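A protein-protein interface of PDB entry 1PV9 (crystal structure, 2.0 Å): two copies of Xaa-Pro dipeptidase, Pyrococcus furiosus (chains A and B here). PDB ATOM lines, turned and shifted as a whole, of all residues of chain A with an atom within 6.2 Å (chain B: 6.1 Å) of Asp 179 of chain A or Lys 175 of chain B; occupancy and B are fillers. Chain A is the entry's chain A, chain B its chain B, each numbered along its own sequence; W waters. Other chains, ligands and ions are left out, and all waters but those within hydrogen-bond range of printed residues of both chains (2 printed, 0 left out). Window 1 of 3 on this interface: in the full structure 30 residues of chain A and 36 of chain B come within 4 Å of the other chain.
The side-chain amino group of Lys 175 of chain B is in salt-bridge range of the side-chain carboxylate of Asp 179 of chain A.
OE1 of Glu 165 of chain A is in salt-bridge range of NZ of Lys 169 of chain B (2.8 Å).
NH1 of Arg 158 of chain A is in salt-bridge range of OE2 of Glu 174 of chain B, at 2.8 Å.
Printed residues of chain B within 4 Å of Arg 158 of chain A: Lys 169, Ala 173 and Glu 174.
Thr 180 of chain A touches none of the printed residues of chain B.
Of the printed residues of chain B, Ala 195 of chain A touches Glu 174.
Of the printed residues of chain A, Lys 169 of chain B touches Arg 158 and Glu 165.
Of the printed residues of chain A, Glu 174 of chain B touches Arg 158 and Ala 195.
Of the printed residues of chain A, Lys 175 of chain B touches Asp 179.
The nearest printed residue of chain B that does not touch Asp 179 of chain A is Leu 37 of chain B (5.1 Å).
The nearest printed residue of chain A that does not touch Lys 169 of chain B is Thr 180 of chain A (5.1 Å).
NZ of Lys 169 of chain B lies close to O of Glu 174 of chain B (3.3 Å).
O of Thr 180 of chain A is in hydrogen-bond range of N of Ala 195 of chain A.
The backbone NH of Leu 213 of chain B lies within hydrogen-bond range of the backbone carbonyl oxygen of Lys 175 of chain B (3.0 Å).
The backbone NH (N) of Ala 173 of chain B lies within hydrogen-bond range of the backbone carbonyl oxygen (O) of Met 168 of chain B (3.1 Å).
The side-chain carboxylate (OE2) of Glu 165 of chain A is in hydrogen-bond range of the side-chain hydroxyl (OG1) of Thr 180 of chain A, 2.6 Å away.
O of Leu 213 of chain B lies within hydrogen-bond range of N of Glu 174 of chain B (2.8 Å).
Of the 11 printed residues of chain A, 4 touch a printed residue of chain B.
Among the printed residues, Asp or Glu carboxylates within 4 Å of a Lys or Arg side-chain nitrogen of the other chain: Arg 158 of chain A with Glu 174 of chain B (2.8 Å), Glu 165 of chain A with Lys 169 of chain B (2.8 Å) and Asp 179 of chain A with Lys 175 of chain B (2.8 Å).
2 positions are printed for both chains.
Of the 6 pairs that touch across the chains among the printed residues, none has its exchanged pair printed and touching as well.
Among the printed residues, pairs that only touch across the chains: Arg 158 of chain A with Lys 169 of chain B, Arg 158 of chain A with Ala 173 of chain B and Ala 195 of chain A with Glu 174 of chain B.
Water W2 lies within hydrogen-bond range of O of Ala 195 of chain A (2.7 Å), OE2 of Glu 174 of chain B (2.8 Å) and NH1 of Arg 158 of chain A (2.8 Å).
Water W1 bridges NZ of Lys 169 of chain B (2.8 Å) and O of Thr 180 of chain A (3.0 Å).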
ATOM      1  N   ARG A 158     -13.262  -2.222  -2.648  1.00  0.00           N
ATOM      2  CA  ARG A 158     -12.464  -3.130  -1.825  1.00  0.00           C
ATOM      3  C   ARG A 158     -11.080  -2.564  -1.514  1.00  0.00           C
ATOM      4  O   ARG A 158     -10.557  -2.756  -0.413  1.00  0.00           O
ATOM      5  CB  ARG A 158     -12.331  -4.488  -2.519  1.00  0.00           C
ATOM      6  CG  ARG A 158     -11.833  -5.603  -1.614  1.00  0.00           C
ATOM      7  CD  ARG A 158     -11.526  -6.919  -2.329  1.00  0.00           C
ATOM      8  NE  ARG A 158     -12.633  -7.385  -3.168  1.00  0.00           N
ATOM      9  CZ  ARG A 158     -13.794  -7.841  -2.706  1.00  0.00           C
ATOM     10  NH1 ARG A 158     -14.029  -7.902  -1.401  1.00  0.00           N
ATOM     11  NH2 ARG A 158     -14.729  -8.239  -3.557  1.00  0.00           N
ATOM     12  N   GLU A 165      -8.403  -0.405   6.584  1.00  0.00           N
ATOM     13  CA  GLU A 165      -8.241  -1.506   7.531  1.00  0.00           C
ATOM     14  C   GLU A 165      -6.770  -1.684   7.917  1.00  0.00           C
ATOM     15  O   GLU A 165      -6.459  -1.986   9.070  1.00  0.00           O
ATOM     16  CB  GLU A 165      -8.852  -2.805   6.988  1.00  0.00           C
ATOM     17  CG  GLU A 165     -10.374  -2.754   6.893  1.00  0.00           C
ATOM     18  CD  GLU A 165     -11.001  -3.996   6.278  1.00  0.00           C
ATOM     19  OE1 GLU A 165     -10.279  -4.838   5.707  1.00  0.00           O
ATOM     20  OE2 GLU A 165     -12.240  -4.125   6.365  1.00  0.00           O
ATOM     21  N   PRO A 176     -10.442  -4.867  12.127  1.00  0.00           N
ATOM     22  CA  PRO A 176     -11.722  -4.162  11.977  1.00  0.00           C
ATOM     23  C   PRO A 176     -12.795  -4.779  12.877  1.00  0.00           C
ATOM     24  O   PRO A 176     -12.730  -5.978  13.162  1.00  0.00           O
ATOM     25  CB  PRO A 176     -12.072  -4.385  10.504  1.00  0.00           C
ATOM     26  CG  PRO A 176     -10.765  -4.660   9.848  1.00  0.00           C
ATOM     27  CD  PRO A 176      -9.978  -5.437  10.847  1.00  0.00           C
ATOM     28  N   ALA A 177     -13.757  -3.970  13.319  1.00  0.00           N
ATOM     29  CA  ALA A 177     -14.844  -4.450  14.171  1.00  0.00           C
ATOM     30  C   ALA A 177     -15.831  -5.311  13.385  1.00  0.00           C
ATOM     31  O   ALA A 177     -16.556  -6.126  13.961  1.00  0.00           O
ATOM     32  CB  ALA A 177     -15.568  -3.280  14.822  1.00  0.00           C
ATOM     33  N   PHE A 178     -15.851  -5.105  12.070  1.00  0.00           N
ATOM     34  CA  PHE A 178     -16.733  -5.820  11.148  1.00  0.00           C
ATOM     35  C   PHE A 178     -16.268  -5.538   9.721  1.00  0.00           C
ATOM     36  O   PHE A 178     -15.458  -4.633   9.498  1.00  0.00           O
ATOM     37  CB  PHE A 178     -18.198  -5.392  11.340  1.00  0.00           C
ATOM     38  CG  PHE A 178     -18.427  -3.911  11.206  1.00  0.00           C
ATOM     39  CD1 PHE A 178     -18.774  -3.353   9.976  1.00  0.00           C
ATOM     40  CD2 PHE A 178     -18.307  -3.070  12.311  1.00  0.00           C
ATOM     41  CE1 PHE A 178     -18.985  -1.982   9.848  1.00  0.00           C
ATOM     42  CE2 PHE A 178     -18.519  -1.702  12.196  1.00  0.00           C
ATOM     43  CZ  PHE A 178     -18.859  -1.156  10.966  1.00  0.00           C
ATOM     44  N   ASP A 179     -16.782  -6.301   8.760  1.00  0.00           N
ATOM     45  CA  ASP A 179     -16.387  -6.131   7.363  1.00  0.00           C
ATOM     46  C   ASP A 179     -16.765  -4.743   6.855  1.00  0.00           C
ATOM     47  O   ASP A 179     -17.943  -4.382   6.813  1.00  0.00           O
ATOM     48  CB  ASP A 179     -16.985  -7.237   6.488  1.00  0.00           C
ATOM     49  CG  ASP A 179     -16.402  -8.603   6.801  1.00  0.00           C
ATOM     50  OD1 ASP A 179     -15.398  -8.674   7.542  1.00  0.00           O
ATOM     51  OD2 ASP A 179     -16.879  -9.664   6.352  1.00  0.00           O
ATOM     52  N   THR A 180     -15.742  -3.973   6.489  1.00  0.00           N
ATOM     53  CA  THR A 180     -15.896  -2.566   6.131  1.00  0.00           C
ATOM     54  C   THR A 180     -16.860  -2.375   4.969  1.00  0.00           C
ATOM     55  O   THR A 180     -16.757  -3.046   3.948  1.00  0.00           O
ATOM     56  CB  THR A 180     -14.520  -1.943   5.811  1.00  0.00           C
ATOM     57  OG1 THR A 180     -13.690  -2.007   6.977  1.00  0.00           O
ATOM     58  CG2 THR A 180     -14.637  -0.447   5.551  1.00  0.00           C
ATOM     59  N   ILE A 181     -17.807  -1.463   5.152  1.00  0.00           N
ATOM     60  CA  ILE A 181     -18.763  -1.133   4.109  1.00  0.00           C
ATOM     61  C   ILE A 181     -18.287   0.103   3.350  1.00  0.00           C
ATOM     62  O   ILE A 181     -18.169   1.189   3.917  1.00  0.00           O
ATOM     63  CB  ILE A 181     -20.185  -0.929   4.705  1.00  0.00           C
ATOM     64  CG1 ILE A 181     -20.780  -2.271   5.154  1.00  0.00           C
ATOM     65  CG2 ILE A 181     -21.117  -0.232   3.704  1.00  0.00           C
ATOM     66  CD1 ILE A 181     -21.657  -2.175   6.390  1.00  0.00           C
ATOM     67  N   VAL A 194     -21.149  -4.349   1.984  1.00  0.00           N
ATOM     68  CA  VAL A 194     -19.716  -4.575   2.192  1.00  0.00           C
ATOM     69  C   VAL A 194     -18.935  -4.258   0.913  1.00  0.00           C
ATOM     70  O   VAL A 194     -19.351  -4.640  -0.187  1.00  0.00           O
ATOM     71  CB  VAL A 194     -19.427  -6.035   2.644  1.00  0.00           C
ATOM     72  CG1 VAL A 194     -17.935  -6.261   2.867  1.00  0.00           C
ATOM     73  CG2 VAL A 194     -20.214  -6.379   3.907  1.00  0.00           C
ATOM     74  N   ALA A 195     -17.817  -3.547   1.066  1.00  0.00           N
ATOM     75  CA  ALA A 195     -16.980  -3.142  -0.065  1.00  0.00           C
ATOM     76  C   ALA A 195     -16.777  -4.290  -1.047  1.00  0.00           C
ATOM     77  O   ALA A 195     -16.379  -5.390  -0.656  1.00  0.00           O
ATOM     78  CB  ALA A 195     -15.641  -2.616   0.425  1.00  0.00           C
ATOM     79  N   ASP A 209     -19.006   2.767   6.163  1.00  0.00           N
ATOM     80  CA  ASP A 209     -19.381   2.233   7.465  1.00  0.00           C
ATOM     81  C   ASP A 209     -18.258   1.334   7.962  1.00  0.00           C
ATOM     82  O   ASP A 209     -18.000   0.278   7.386  1.00  0.00           O
ATOM     83  CB  ASP A 209     -20.696   1.446   7.354  1.00  0.00           C
ATOM     84  CG  ASP A 209     -21.371   1.221   8.699  1.00  0.00           C
ATOM     85  OD1 ASP A 209     -20.691   1.274   9.745  1.00  0.00           O
ATOM     86  OD2 ASP A 209     -22.595   0.992   8.810  1.00  0.00           O
ATOM     87  N   LEU B  37     -25.640 -10.422   5.912  1.00  0.00           N
ATOM     88  CA  LEU B  37     -24.917 -10.099   7.144  1.00  0.00           C
ATOM     89  C   LEU B  37     -25.841  -9.918   8.354  1.00  0.00           C
ATOM     90  O   LEU B  37     -25.558 -10.434   9.439  1.00  0.00           O
ATOM     91  CB  LEU B  37     -24.053  -8.848   6.931  1.00  0.00           C
ATOM     92  CG  LEU B  37     -23.064  -8.416   8.018  1.00  0.00           C
ATOM     93  CD1 LEU B  37     -21.748  -9.177   7.911  1.00  0.00           C
ATOM     94  CD2 LEU B  37     -22.818  -6.920   7.935  1.00  0.00           C
ATOM     95  N   MET B 168      -3.558  -9.355   0.472  1.00  0.00           N
ATOM     96  CA  MET B 168      -4.596 -10.338   0.171  1.00  0.00           C
ATOM     97  C   MET B 168      -5.887  -9.675  -0.304  1.00  0.00           C
ATOM     98  O   MET B 168      -6.506 -10.130  -1.267  1.00  0.00           O
ATOM     99  CB  MET B 168      -4.875 -11.223   1.389  1.00  0.00           C
ATOM    100  CG  MET B 168      -3.797 -12.262   1.662  1.00  0.00           C
ATOM    101  SD  MET B 168      -4.368 -13.664   2.653  1.00  0.00           S
ATOM    102  CE  MET B 168      -4.502 -12.908   4.272  1.00  0.00           C
ATOM    103  N   LYS B 169      -6.282  -8.598   0.372  1.00  0.00           N
ATOM    104  CA  LYS B 169      -7.496  -7.867   0.017  1.00  0.00           C
ATOM    105  C   LYS B 169      -7.339  -7.139  -1.318  1.00  0.00           C
ATOM    106  O   LYS B 169      -8.269  -7.105  -2.122  1.00  0.00           O
ATOM    107  CB  LYS B 169      -7.892  -6.889   1.127  1.00  0.00           C
ATOM    108  CG  LYS B 169      -9.322  -6.373   1.015  1.00  0.00           C
ATOM    109  CD  LYS B 169      -9.817  -5.789   2.326  1.00  0.00           C
ATOM    110  CE  LYS B 169     -10.855  -6.688   2.962  1.00  0.00           C
ATOM    111  NZ  LYS B 169     -11.879  -5.934   3.739  1.00  0.00           N
ATOM    112  N   ALA B 173      -9.408 -10.864  -2.207  1.00  0.00           N
ATOM    113  CA  ALA B 173      -9.958 -11.570  -1.049  1.00  0.00           C
ATOM    114  C   ALA B 173     -10.885 -10.673  -0.231  1.00  0.00           C
ATOM    115  O   ALA B 173     -10.619  -9.481  -0.053  1.00  0.00           O
ATOM    116  CB  ALA B 173      -8.845 -12.122  -0.171  1.00  0.00           C
ATOM    117  N   GLU B 174     -11.975 -11.260   0.256  1.00  0.00           N
ATOM    118  CA  GLU B 174     -12.928 -10.555   1.105  1.00  0.00           C
ATOM    119  C   GLU B 174     -12.281 -10.157   2.426  1.00  0.00           C
ATOM    120  O   GLU B 174     -12.542  -9.078   2.952  1.00  0.00           O
ATOM    121  CB  GLU B 174     -14.157 -11.431   1.362  1.00  0.00           C
ATOM    122  CG  GLU B 174     -15.459 -10.661   1.516  1.00  0.00           C
ATOM    123  CD  GLU B 174     -15.983 -10.097   0.209  1.00  0.00           C
ATOM    124  OE1 GLU B 174     -16.239 -10.884  -0.732  1.00  0.00           O
ATOM    125  OE2 GLU B 174     -16.147  -8.860   0.123  1.00  0.00           O
ATOM    126  N   LYS B 175     -11.436 -11.047   2.945  1.00  0.00           N
ATOM    127  CA  LYS B 175     -10.704 -10.849   4.194  1.00  0.00           C
ATOM    128  C   LYS B 175      -9.773 -12.047   4.407  1.00  0.00           C
ATOM    129  O   LYS B 175      -9.793 -12.985   3.605  1.00  0.00           O
ATOM    130  CB  LYS B 175     -11.667 -10.671   5.383  1.00  0.00           C
ATOM    131  CG  LYS B 175     -12.615 -11.834   5.648  1.00  0.00           C
ATOM    132  CD  LYS B 175     -13.523 -11.525   6.832  1.00  0.00           C
ATOM    133  CE  LYS B 175     -14.638 -12.549   6.962  1.00  0.00           C
ATOM    134  NZ  LYS B 175     -15.816 -12.214   6.104  1.00  0.00           N
ATOM    135  N   PRO B 176      -8.953 -12.028   5.459  1.00  0.00           N
ATOM    136  CA  PRO B 176      -8.154 -13.208   5.807  1.00  0.00           C
ATOM    137  C   PRO B 176      -9.061 -14.329   6.306  1.00  0.00           C
ATOM    138  O   PRO B 176     -10.083 -14.046   6.934  1.00  0.00           O
ATOM    139  CB  PRO B 176      -7.253 -12.708   6.944  1.00  0.00           C
ATOM    140  CG  PRO B 176      -7.347 -11.224   6.895  1.00  0.00           C
ATOM    141  CD  PRO B 176      -8.710 -10.910   6.389  1.00  0.00           C
ATOM    142  N   ALA B 177      -8.692 -15.575   6.021  1.00  0.00           N
ATOM    143  CA  ALA B 177      -9.470 -16.739   6.443  1.00  0.00           C
ATOM    144  C   ALA B 177      -9.471 -16.916   7.965  1.00  0.00           C
ATOM    145  O   ALA B 177     -10.394 -17.507   8.527  1.00  0.00           O
ATOM    146  CB  ALA B 177      -8.949 -17.992   5.762  1.00  0.00           C
ATOM    147  N   GLY B 211      -4.332 -17.460   5.634  1.00  0.00           N
ATOM    148  CA  GLY B 211      -5.314 -17.953   4.690  1.00  0.00           C
ATOM    149  C   GLY B 211      -6.117 -16.828   4.076  1.00  0.00           C
ATOM    150  O   GLY B 211      -6.226 -15.747   4.653  1.00  0.00           O
ATOM    151  N   ALA B 212      -6.676 -17.085   2.900  1.00  0.00           N
ATOM    152  CA  ALA B 212      -7.522 -16.111   2.230  1.00  0.00           C
ATOM    153  C   ALA B 212      -8.952 -16.616   2.140  1.00  0.00           C
ATOM    154  O   ALA B 212      -9.191 -17.783   1.814  1.00  0.00           O
ATOM    155  CB  ALA B 212      -6.982 -15.799   0.840  1.00  0.00           C
ATOM    156  N   LEU B 213      -9.896 -15.734   2.452  1.00  0.00           N
ATOM    157  CA  LEU B 213     -11.295 -15.970   2.140  1.00  0.00           C
ATOM    158  C   LEU B 213     -11.608 -15.232   0.845  1.00  0.00           C
ATOM    159  O   LEU B 213     -11.606 -13.996   0.802  1.00  0.00           O
ATOM    160  CB  LEU B 213     -12.210 -15.500   3.278  1.00  0.00           C
ATOM    161  CG  LEU B 213     -13.722 -15.596   3.039  1.00  0.00           C
ATOM    162  CD1 LEU B 213     -14.204 -17.034   3.116  1.00  0.00           C
ATOM    163  CD2 LEU B 213     -14.481 -14.722   4.033  1.00  0.00           C
ATOM    164  N   TYR B 214     -11.850 -15.999  -0.212  1.00  0.00           N
ATOM    165  CA  TYR B 214     -12.134 -15.446  -1.529  1.00  0.00           C
ATOM    166  C   TYR B 214     -13.425 -16.051  -2.056  1.00  0.00           C
ATOM    167  O   TYR B 214     -13.557 -17.274  -2.125  1.00  0.00           O
ATOM    168  CB  TYR B 214     -10.976 -15.735  -2.496  1.00  0.00           C
ATOM    169  CG  TYR B 214     -11.261 -15.352  -3.934  1.00  0.00           C
ATOM    170  CD1 TYR B 214     -11.063 -14.045  -4.380  1.00  0.00           C
ATOM    171  CD2 TYR B 214     -11.731 -16.296  -4.850  1.00  0.00           C
ATOM    172  CE1 TYR B 214     -11.326 -13.686  -5.699  1.00  0.00           C
ATOM    173  CE2 TYR B 214     -12.001 -15.946  -6.169  1.00  0.00           C
ATOM    174  CZ  TYR B 214     -11.795 -14.640  -6.585  1.00  0.00           C
ATOM    175  OH  TYR B 214     -12.053 -14.287  -7.886  1.00  0.00           O
HETATM  176  O   HOH W   1     -14.532  -5.008   3.498  1.00  0.00           O
HETATM  177  O   HOH W   2     -14.669  -6.659   1.049  1.00  0.00           O
